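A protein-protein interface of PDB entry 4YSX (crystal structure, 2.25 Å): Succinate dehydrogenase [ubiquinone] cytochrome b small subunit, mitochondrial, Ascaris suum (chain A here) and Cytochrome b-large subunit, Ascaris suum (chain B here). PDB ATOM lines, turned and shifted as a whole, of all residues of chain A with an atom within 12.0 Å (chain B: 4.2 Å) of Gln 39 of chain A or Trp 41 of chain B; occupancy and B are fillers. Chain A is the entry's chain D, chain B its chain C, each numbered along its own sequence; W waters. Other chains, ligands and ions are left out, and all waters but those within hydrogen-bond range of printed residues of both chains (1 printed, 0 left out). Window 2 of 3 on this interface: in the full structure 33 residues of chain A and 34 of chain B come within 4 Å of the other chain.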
ATOM      1  N   ALA A  35      -9.099  11.184  14.004  1.00  0.00           N
ATOM      2  CA  ALA A  35      -9.461  10.804  12.643  1.00  0.00           C
ATOM      3  C   ALA A  35      -8.788  11.782  11.680  1.00  0.00           C
ATOM      4  O   ALA A  35      -8.304  12.845  12.081  1.00  0.00           O
ATOM      5  CB  ALA A  35     -10.967  10.835  12.465  1.00  0.00           C
ATOM      6  N   ALA A  36      -8.757  11.417  10.405  1.00  0.00           N
ATOM      7  CA  ALA A  36      -8.204  12.297   9.374  1.00  0.00           C
ATOM      8  C   ALA A  36      -9.040  13.574   9.291  1.00  0.00           C
ATOM      9  O   ALA A  36     -10.240  13.538   9.541  1.00  0.00           O
ATOM     10  CB  ALA A  36      -8.191  11.589   8.020  1.00  0.00           C
ATOM     11  N   PRO A  37      -8.414  14.706   8.919  1.00  0.00           N
ATOM     12  CA  PRO A  37      -9.215  15.914   8.704  1.00  0.00           C
ATOM     13  C   PRO A  37     -10.183  15.760   7.532  1.00  0.00           C
ATOM     14  O   PRO A  37     -10.034  14.841   6.731  1.00  0.00           O
ATOM     15  CB  PRO A  37      -8.169  17.003   8.413  1.00  0.00           C
ATOM     16  CG  PRO A  37      -6.931  16.283   8.054  1.00  0.00           C
ATOM     17  CD  PRO A  37      -6.976  14.961   8.769  1.00  0.00           C
ATOM     18  N   PRO A  38     -11.185  16.646   7.443  1.00  0.00           N
ATOM     19  CA  PRO A  38     -12.019  16.652   6.248  1.00  0.00           C
ATOM     20  C   PRO A  38     -11.154  17.056   5.048  1.00  0.00           C
ATOM     21  O   PRO A  38     -10.420  18.042   5.117  1.00  0.00           O
ATOM     22  CB  PRO A  38     -13.077  17.710   6.559  1.00  0.00           C
ATOM     23  CG  PRO A  38     -12.414  18.642   7.524  1.00  0.00           C
ATOM     24  CD  PRO A  38     -11.433  17.813   8.311  1.00  0.00           C
ATOM     25  N   GLN A  39     -11.212  16.269   3.982  1.00  0.00           N
ATOM     26  CA  GLN A  39     -10.348  16.471   2.834  1.00  0.00           C
ATOM     27  C   GLN A  39     -11.042  15.891   1.616  1.00  0.00           C
ATOM     28  O   GLN A  39     -11.417  14.723   1.615  1.00  0.00           O
ATOM     29  CB  GLN A  39      -8.994  15.774   3.056  1.00  0.00           C
ATOM     30  CG  GLN A  39      -8.058  15.848   1.858  1.00  0.00           C
ATOM     31  CD  GLN A  39      -6.648  15.334   2.129  1.00  0.00           C
ATOM     32  OE1 GLN A  39      -6.139  15.426   3.247  1.00  0.00           O
ATOM     33  NE2 GLN A  39      -6.001  14.801   1.086  1.00  0.00           N
ATOM     34  N   PHE A  40     -11.219  16.698   0.583  1.00  0.00           N
ATOM     35  CA  PHE A  40     -11.904  16.212  -0.610  1.00  0.00           C
ATOM     36  C   PHE A  40     -10.981  15.342  -1.453  1.00  0.00           C
ATOM     37  O   PHE A  40      -9.977  15.816  -1.989  1.00  0.00           O
ATOM     38  CB  PHE A  40     -12.445  17.346  -1.460  1.00  0.00           C
ATOM     39  CG  PHE A  40     -13.225  16.873  -2.644  1.00  0.00           C
ATOM     40  CD1 PHE A  40     -14.527  16.451  -2.498  1.00  0.00           C
ATOM     41  CD2 PHE A  40     -12.644  16.823  -3.904  1.00  0.00           C
ATOM     42  CE1 PHE A  40     -15.250  16.015  -3.589  1.00  0.00           C
ATOM     43  CE2 PHE A  40     -13.369  16.391  -5.004  1.00  0.00           C
ATOM     44  CZ  PHE A  40     -14.673  15.985  -4.850  1.00  0.00           C
ATOM     45  N   ASP A  41     -11.359  14.074  -1.576  1.00  0.00           N
ATOM     46  CA  ASP A  41     -10.626  13.111  -2.359  1.00  0.00           C
ATOM     47  C   ASP A  41     -11.189  13.070  -3.765  1.00  0.00           C
ATOM     48  O   ASP A  41     -12.237  12.480  -3.992  1.00  0.00           O
ATOM     49  CB  ASP A  41     -10.759  11.743  -1.720  1.00  0.00           C
ATOM     50  CG  ASP A  41      -9.831  10.724  -2.331  1.00  0.00           C
ATOM     51  OD1 ASP A  41      -9.301  10.957  -3.451  1.00  0.00           O
ATOM     52  OD2 ASP A  41      -9.644   9.684  -1.670  1.00  0.00           O
ATOM     53  N   PRO A  42     -10.483  13.672  -4.727  1.00  0.00           N
ATOM     54  CA  PRO A  42     -11.067  13.788  -6.064  1.00  0.00           C
ATOM     55  C   PRO A  42     -11.179  12.476  -6.837  1.00  0.00           C
ATOM     56  O   PRO A  42     -11.944  12.398  -7.798  1.00  0.00           O
ATOM     57  CB  PRO A  42     -10.125  14.750  -6.773  1.00  0.00           C
ATOM     58  CG  PRO A  42      -8.821  14.577  -6.083  1.00  0.00           C
ATOM     59  CD  PRO A  42      -9.119  14.206  -4.667  1.00  0.00           C
ATOM     60  N   ILE A  43     -10.417  11.475  -6.434  1.00  0.00           N
ATOM     61  CA  ILE A  43     -10.458  10.164  -7.077  1.00  0.00           C
ATOM     62  C   ILE A  43     -11.540   9.292  -6.446  1.00  0.00           C
ATOM     63  O   ILE A  43     -12.360   8.731  -7.158  1.00  0.00           O
ATOM     64  CB  ILE A  43      -9.070   9.501  -7.039  1.00  0.00           C
ATOM     65  CG1 ILE A  43      -8.198  10.176  -8.106  1.00  0.00           C
ATOM     66  CG2 ILE A  43      -9.163   7.993  -7.283  1.00  0.00           C
ATOM     67  CD1 ILE A  43      -6.717   9.972  -7.931  1.00  0.00           C
ATOM     68  N   ALA A  44     -11.547   9.210  -5.116  1.00  0.00           N
ATOM     69  CA  ALA A  44     -12.602   8.502  -4.373  1.00  0.00           C
ATOM     70  C   ALA A  44     -14.005   9.060  -4.638  1.00  0.00           C
ATOM     71  O   ALA A  44     -14.977   8.307  -4.691  1.00  0.00           O
ATOM     72  CB  ALA A  44     -12.310   8.527  -2.880  1.00  0.00           C
ATOM     73  N   ALA A  45     -14.106  10.376  -4.797  1.00  0.00           N
ATOM     74  CA  ALA A  45     -15.382  11.021  -5.112  1.00  0.00           C
ATOM     75  C   ALA A  45     -15.849  10.693  -6.534  1.00  0.00           C
ATOM     76  O   ALA A  45     -17.049  10.666  -6.806  1.00  0.00           O
ATOM     77  CB  ALA A  45     -15.263  12.523  -4.934  1.00  0.00           C
ATOM     78  N   GLU A  46     -14.890  10.437  -7.422  1.00  0.00           N
ATOM     79  CA  GLU A  46     -15.158  10.088  -8.817  1.00  0.00           C
ATOM     80  C   GLU A  46     -15.678   8.647  -9.022  1.00  0.00           C
ATOM     81  O   GLU A  46     -16.172   8.328 -10.104  1.00  0.00           O
ATOM     82  CB  GLU A  46     -13.881  10.296  -9.650  1.00  0.00           C
ATOM     83  CG  GLU A  46     -14.102  10.473 -11.145  1.00  0.00           C
ATOM     84  CD  GLU A  46     -14.550  11.871 -11.537  1.00  0.00           C
ATOM     85  OE1 GLU A  46     -14.468  12.194 -12.741  1.00  0.00           O
ATOM     86  OE2 GLU A  46     -14.987  12.650 -10.664  1.00  0.00           O
ATOM     87  N   PHE A  49     -19.503   8.117 -10.197  1.00  0.00           N
ATOM     88  CA  PHE A  49     -20.102   9.422 -10.512  1.00  0.00           C
ATOM     89  C   PHE A  49     -20.579   9.461 -11.970  1.00  0.00           C
ATOM     90  O   PHE A  49     -19.774   9.592 -12.895  1.00  0.00           O
ATOM     91  CB  PHE A  49     -19.093  10.554 -10.222  1.00  0.00           C
ATOM     92  CG  PHE A  49     -19.466  11.898 -10.807  1.00  0.00           C
ATOM     93  CD1 PHE A  49     -18.760  12.420 -11.892  1.00  0.00           C
ATOM     94  CD2 PHE A  49     -20.504  12.648 -10.269  1.00  0.00           C
ATOM     95  CE1 PHE A  49     -19.089  13.655 -12.432  1.00  0.00           C
ATOM     96  CE2 PHE A  49     -20.838  13.885 -10.803  1.00  0.00           C
ATOM     97  CZ  PHE A  49     -20.129  14.389 -11.886  1.00  0.00           C
ATOM     98  N   LEU A  52     -24.034  14.678 -14.391  1.00  0.00           N
ATOM     99  CA  LEU A  52     -25.370  15.280 -14.359  1.00  0.00           C
ATOM    100  C   LEU A  52     -25.678  15.859 -15.736  1.00  0.00           C
ATOM    101  O   LEU A  52     -24.758  16.138 -16.510  1.00  0.00           O
ATOM    102  CB  LEU A  52     -25.457  16.379 -13.293  1.00  0.00           C
ATOM    103  CG  LEU A  52     -24.891  16.050 -11.901  1.00  0.00           C
ATOM    104  CD1 LEU A  52     -23.485  16.610 -11.734  1.00  0.00           C
ATOM    105  CD2 LEU A  52     -25.790  16.586 -10.797  1.00  0.00           C
ATOM    106  N   PHE A 111     -28.945  27.329   2.688  1.00  0.00           N
ATOM    107  CA  PHE A 111     -28.123  27.685   3.857  1.00  0.00           C
ATOM    108  C   PHE A 111     -28.764  28.782   4.702  1.00  0.00           C
ATOM    109  O   PHE A 111     -28.631  28.771   5.895  1.00  0.00           O
ATOM    110  CB  PHE A 111     -26.701  28.109   3.449  1.00  0.00           C
ATOM    111  CG  PHE A 111     -25.775  28.357   4.626  1.00  0.00           C
ATOM    112  CD1 PHE A 111     -25.317  27.297   5.408  1.00  0.00           C
ATOM    113  CD2 PHE A 111     -25.373  29.645   4.958  1.00  0.00           C
ATOM    114  CE1 PHE A 111     -24.467  27.519   6.487  1.00  0.00           C
ATOM    115  CE2 PHE A 111     -24.526  29.874   6.036  1.00  0.00           C
ATOM    116  CZ  PHE A 111     -24.069  28.808   6.796  1.00  0.00           C
ATOM    117  N   PRO B  37     -19.953  15.589  -6.438  1.00  0.00           N
ATOM    118  CA  PRO B  37     -19.382  15.306  -5.126  1.00  0.00           C
ATOM    119  C   PRO B  37     -18.824  16.547  -4.410  1.00  0.00           C
ATOM    120  O   PRO B  37     -19.009  16.667  -3.202  1.00  0.00           O
ATOM    121  CB  PRO B  37     -18.277  14.292  -5.428  1.00  0.00           C
ATOM    122  CG  PRO B  37     -18.692  13.634  -6.694  1.00  0.00           C
ATOM    123  CD  PRO B  37     -19.424  14.690  -7.480  1.00  0.00           C
ATOM    124  N   ILE B  38     -18.181  17.461  -5.145  1.00  0.00           N
ATOM    125  CA  ILE B  38     -17.636  18.674  -4.524  1.00  0.00           C
ATOM    126  C   ILE B  38     -18.740  19.555  -3.963  1.00  0.00           C
ATOM    127  O   ILE B  38     -18.560  20.169  -2.906  1.00  0.00           O
ATOM    128  CB  ILE B  38     -16.672  19.474  -5.452  1.00  0.00           C
ATOM    129  CG1 ILE B  38     -15.961  20.585  -4.662  1.00  0.00           C
ATOM    130  CG2 ILE B  38     -17.377  20.079  -6.650  1.00  0.00           C
ATOM    131  CD1 ILE B  38     -15.167  20.077  -3.475  1.00  0.00           C
ATOM    132  N   GLN B  39     -19.890  19.593  -4.630  1.00  0.00           N
ATOM    133  CA  GLN B  39     -21.061  20.329  -4.101  1.00  0.00           C
ATOM    134  C   GLN B  39     -21.609  19.716  -2.814  1.00  0.00           C
ATOM    135  O   GLN B  39     -22.018  20.442  -1.889  1.00  0.00           O
ATOM    136  CB  GLN B  39     -22.161  20.395  -5.150  1.00  0.00           C
ATOM    137  CG  GLN B  39     -21.823  21.319  -6.308  1.00  0.00           C
ATOM    138  CD  GLN B  39     -22.768  21.183  -7.480  1.00  0.00           C
ATOM    139  OE1 GLN B  39     -23.451  20.164  -7.628  1.00  0.00           O
ATOM    140  NE2 GLN B  39     -22.825  22.220  -8.321  1.00  0.00           N
ATOM    141  N   VAL B  40     -21.634  18.383  -2.754  1.00  0.00           N
ATOM    142  CA  VAL B  40     -21.993  17.688  -1.517  1.00  0.00           C
ATOM    143  C   VAL B  40     -20.967  18.007  -0.426  1.00  0.00           C
ATOM    144  O   VAL B  40     -21.332  18.292   0.721  1.00  0.00           O
ATOM    145  CB  VAL B  40     -22.072  16.151  -1.682  1.00  0.00           C
ATOM    146  CG1 VAL B  40     -22.253  15.462  -0.326  1.00  0.00           C
ATOM    147  CG2 VAL B  40     -23.210  15.768  -2.621  1.00  0.00           C
ATOM    148  N   TRP B  41     -19.688  17.941  -0.776  1.00  0.00           N
ATOM    149  CA  TRP B  41     -18.636  18.212   0.192  1.00  0.00           C
ATOM    150  C   TRP B  41     -18.807  19.633   0.737  1.00  0.00           C
ATOM    151  O   TRP B  41     -18.643  19.875   1.940  1.00  0.00           O
ATOM    152  CB  TRP B  41     -17.267  18.034  -0.454  1.00  0.00           C
ATOM    153  CG  TRP B  41     -16.133  17.992   0.516  1.00  0.00           C
ATOM    154  CD1 TRP B  41     -15.522  16.876   1.004  1.00  0.00           C
ATOM    155  CD2 TRP B  41     -15.446  19.118   1.107  1.00  0.00           C
ATOM    156  NE1 TRP B  41     -14.506  17.233   1.871  1.00  0.00           N
ATOM    157  CE2 TRP B  41     -14.439  18.602   1.945  1.00  0.00           C
ATOM    158  CE3 TRP B  41     -15.596  20.510   1.018  1.00  0.00           C
ATOM    159  CZ2 TRP B  41     -13.584  19.427   2.686  1.00  0.00           C
ATOM    160  CZ3 TRP B  41     -14.736  21.333   1.755  1.00  0.00           C
ATOM    161  CH2 TRP B  41     -13.748  20.784   2.576  1.00  0.00           C
ATOM    162  N   GLY B  42     -19.170  20.556  -0.155  1.00  0.00           N
ATOM    163  CA  GLY B  42     -19.303  21.970   0.187  1.00  0.00           C
ATOM    164  C   GLY B  42     -20.475  22.288   1.091  1.00  0.00           C
ATOM    165  O   GLY B  42     -20.391  23.187   1.928  1.00  0.00           O
ATOM    166  N   TRP B  43     -21.578  21.573   0.918  1.00  0.00           N
ATOM    167  CA  TRP B  43     -22.674  21.658   1.881  1.00  0.00           C
ATOM    168  C   TRP B  43     -22.222  21.242   3.270  1.00  0.00           C
ATOM    169  O   TRP B  43     -22.459  21.974   4.238  1.00  0.00           O
ATOM    170  CB  TRP B  43     -23.882  20.808   1.482  1.00  0.00           C
ATOM    171  CG  TRP B  43     -24.995  20.984   2.468  1.00  0.00           C
ATOM    172  CD1 TRP B  43     -25.350  20.126   3.481  1.00  0.00           C
ATOM    173  CD2 TRP B  43     -25.850  22.122   2.587  1.00  0.00           C
ATOM    174  NE1 TRP B  43     -26.396  20.660   4.206  1.00  0.00           N
ATOM    175  CE2 TRP B  43     -26.724  21.880   3.676  1.00  0.00           C
ATOM    176  CE3 TRP B  43     -25.978  23.317   1.862  1.00  0.00           C
ATOM    177  CZ2 TRP B  43     -27.699  22.789   4.063  1.00  0.00           C
ATOM    178  CZ3 TRP B  43     -26.933  24.218   2.251  1.00  0.00           C
ATOM    179  CH2 TRP B  43     -27.788  23.955   3.353  1.00  0.00           C
ATOM    180  N   ASP B  44     -21.570  20.078   3.374  1.00  0.00           N
ATOM    181  CA  ASP B  44     -21.120  19.571   4.682  1.00  0.00           C
ATOM    182  C   ASP B  44     -20.116  20.527   5.327  1.00  0.00           C
ATOM    183  O   ASP B  44     -20.055  20.613   6.558  1.00  0.00           O
ATOM    184  CB  ASP B  44     -20.531  18.153   4.588  1.00  0.00           C
ATOM    185  CG  ASP B  44     -21.569  17.099   4.128  1.00  0.00           C
ATOM    186  OD1 ASP B  44     -21.164  15.957   3.820  1.00  0.00           O
ATOM    187  OD2 ASP B  44     -22.782  17.404   4.048  1.00  0.00           O
ATOM    188  N   TYR B  45     -19.344  21.230   4.486  1.00  0.00           N
ATOM    189  CA  TYR B  45     -18.429  22.289   4.925  1.00  0.00           C
ATOM    190  C   TYR B  45     -19.198  23.472   5.513  1.00  0.00           C
ATOM    191  O   TYR B  45     -18.871  23.951   6.585  1.00  0.00           O
ATOM    192  CB  TYR B  45     -17.518  22.772   3.758  1.00  0.00           C
ATOM    193  CG  TYR B  45     -16.699  23.999   4.104  1.00  0.00           C
ATOM    194  CD1 TYR B  45     -15.451  23.883   4.723  1.00  0.00           C
ATOM    195  CD2 TYR B  45     -17.185  25.275   3.844  1.00  0.00           C
ATOM    196  CE1 TYR B  45     -14.707  25.013   5.054  1.00  0.00           C
ATOM    197  CE2 TYR B  45     -16.454  26.408   4.163  1.00  0.00           C
ATOM    198  CZ  TYR B  45     -15.223  26.277   4.768  1.00  0.00           C
ATOM    199  OH  TYR B  45     -14.512  27.409   5.096  1.00  0.00           O
HETATM  200  O   HOH W   1     -13.829  14.670   3.673  1.00  0.00           O
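Among the printed residues, pairs that only touch across the chains: Gln 39 of chain A with Trp 41 of chain B (3.7 Å), Phe 40 of chain A with Pro 37 of chain B (3.7 Å), Phe 40 of chain A with Ile 38 of chain B (3.6 Å), Phe 40 of chain A with Trp 41 of chain B (3.6 Å), Ala 45 of chain A with Pro 37 of chain B (3.4 Å), Phe 49 of chain A with Pro 37 of chain B (3.6 Å) and Phe 111 of chain A with Trp 43 of chain B (3.6 Å).
Gln 39 of chain A touches just one residue of chain B: Trp 41.
Pro 37 of chain B touches just these residues of chain A: Phe 40, Ala 45 and Phe 49.
Ile 38 of chain B touches just one residue of chain A: Phe 40.
No residue of chain A comes within 4 Å of Asp 44 of chain B.
No residue of chain A comes within 4 Å of Tyr 45 of chain B.
Printed residues of chain B within 4 Å of Phe 49 of chain A: Pro 37.
Of the printed residues of chain A, Trp 43 of chain B touches Phe 111 (3.6 Å).
Printed residues of chain B within 4 Å of Phe 40 of chain A: Pro 37, Ile 38 and Trp 41.
Printed residues of chain B within 4 Å of Phe 111 of chain A: Trp 43.
Printed residues of chain B within 4 Å of Ala 45 of chain A: Pro 37.
Asp 41 of chain A touches none of the printed residues of chain B.
The nearest printed residue of chain B that does not touch Gln 39 of chain A is Ile 38 of chain B (7.8 Å).
The nearest residue of chain A that does not touch Trp 41 of chain B is Pro 38 of chain A (4.1 Å).
The nearest printed residue of chain B that does not touch Ala 45 of chain A is Ile 38 of chain B (5.7 Å).
Of the 9 printed residues of chain B, 4 touch a printed residue of chain A.
Hydrophobic or aromatic side chains of chain B that line the printed part of chain A: Pro 37, Ile 38, Trp 41 and Trp 43.
Printed residues of chain A that touch a printed residue of chain B: Gln 39, Phe 40, Ala 45, Phe 49 and Phe 111.
Among the printed residues, 7 pairs touch across the chains.
Among the printed residues, no Asp or Glu carboxylate lies within 4 Å of a Lys or Arg side-chain nitrogen of the other chain.
Water W1 bridges N of Gln 39 of chain A (3.1 Å) and NE1 of Trp 41 of chain B (3.2 Å).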
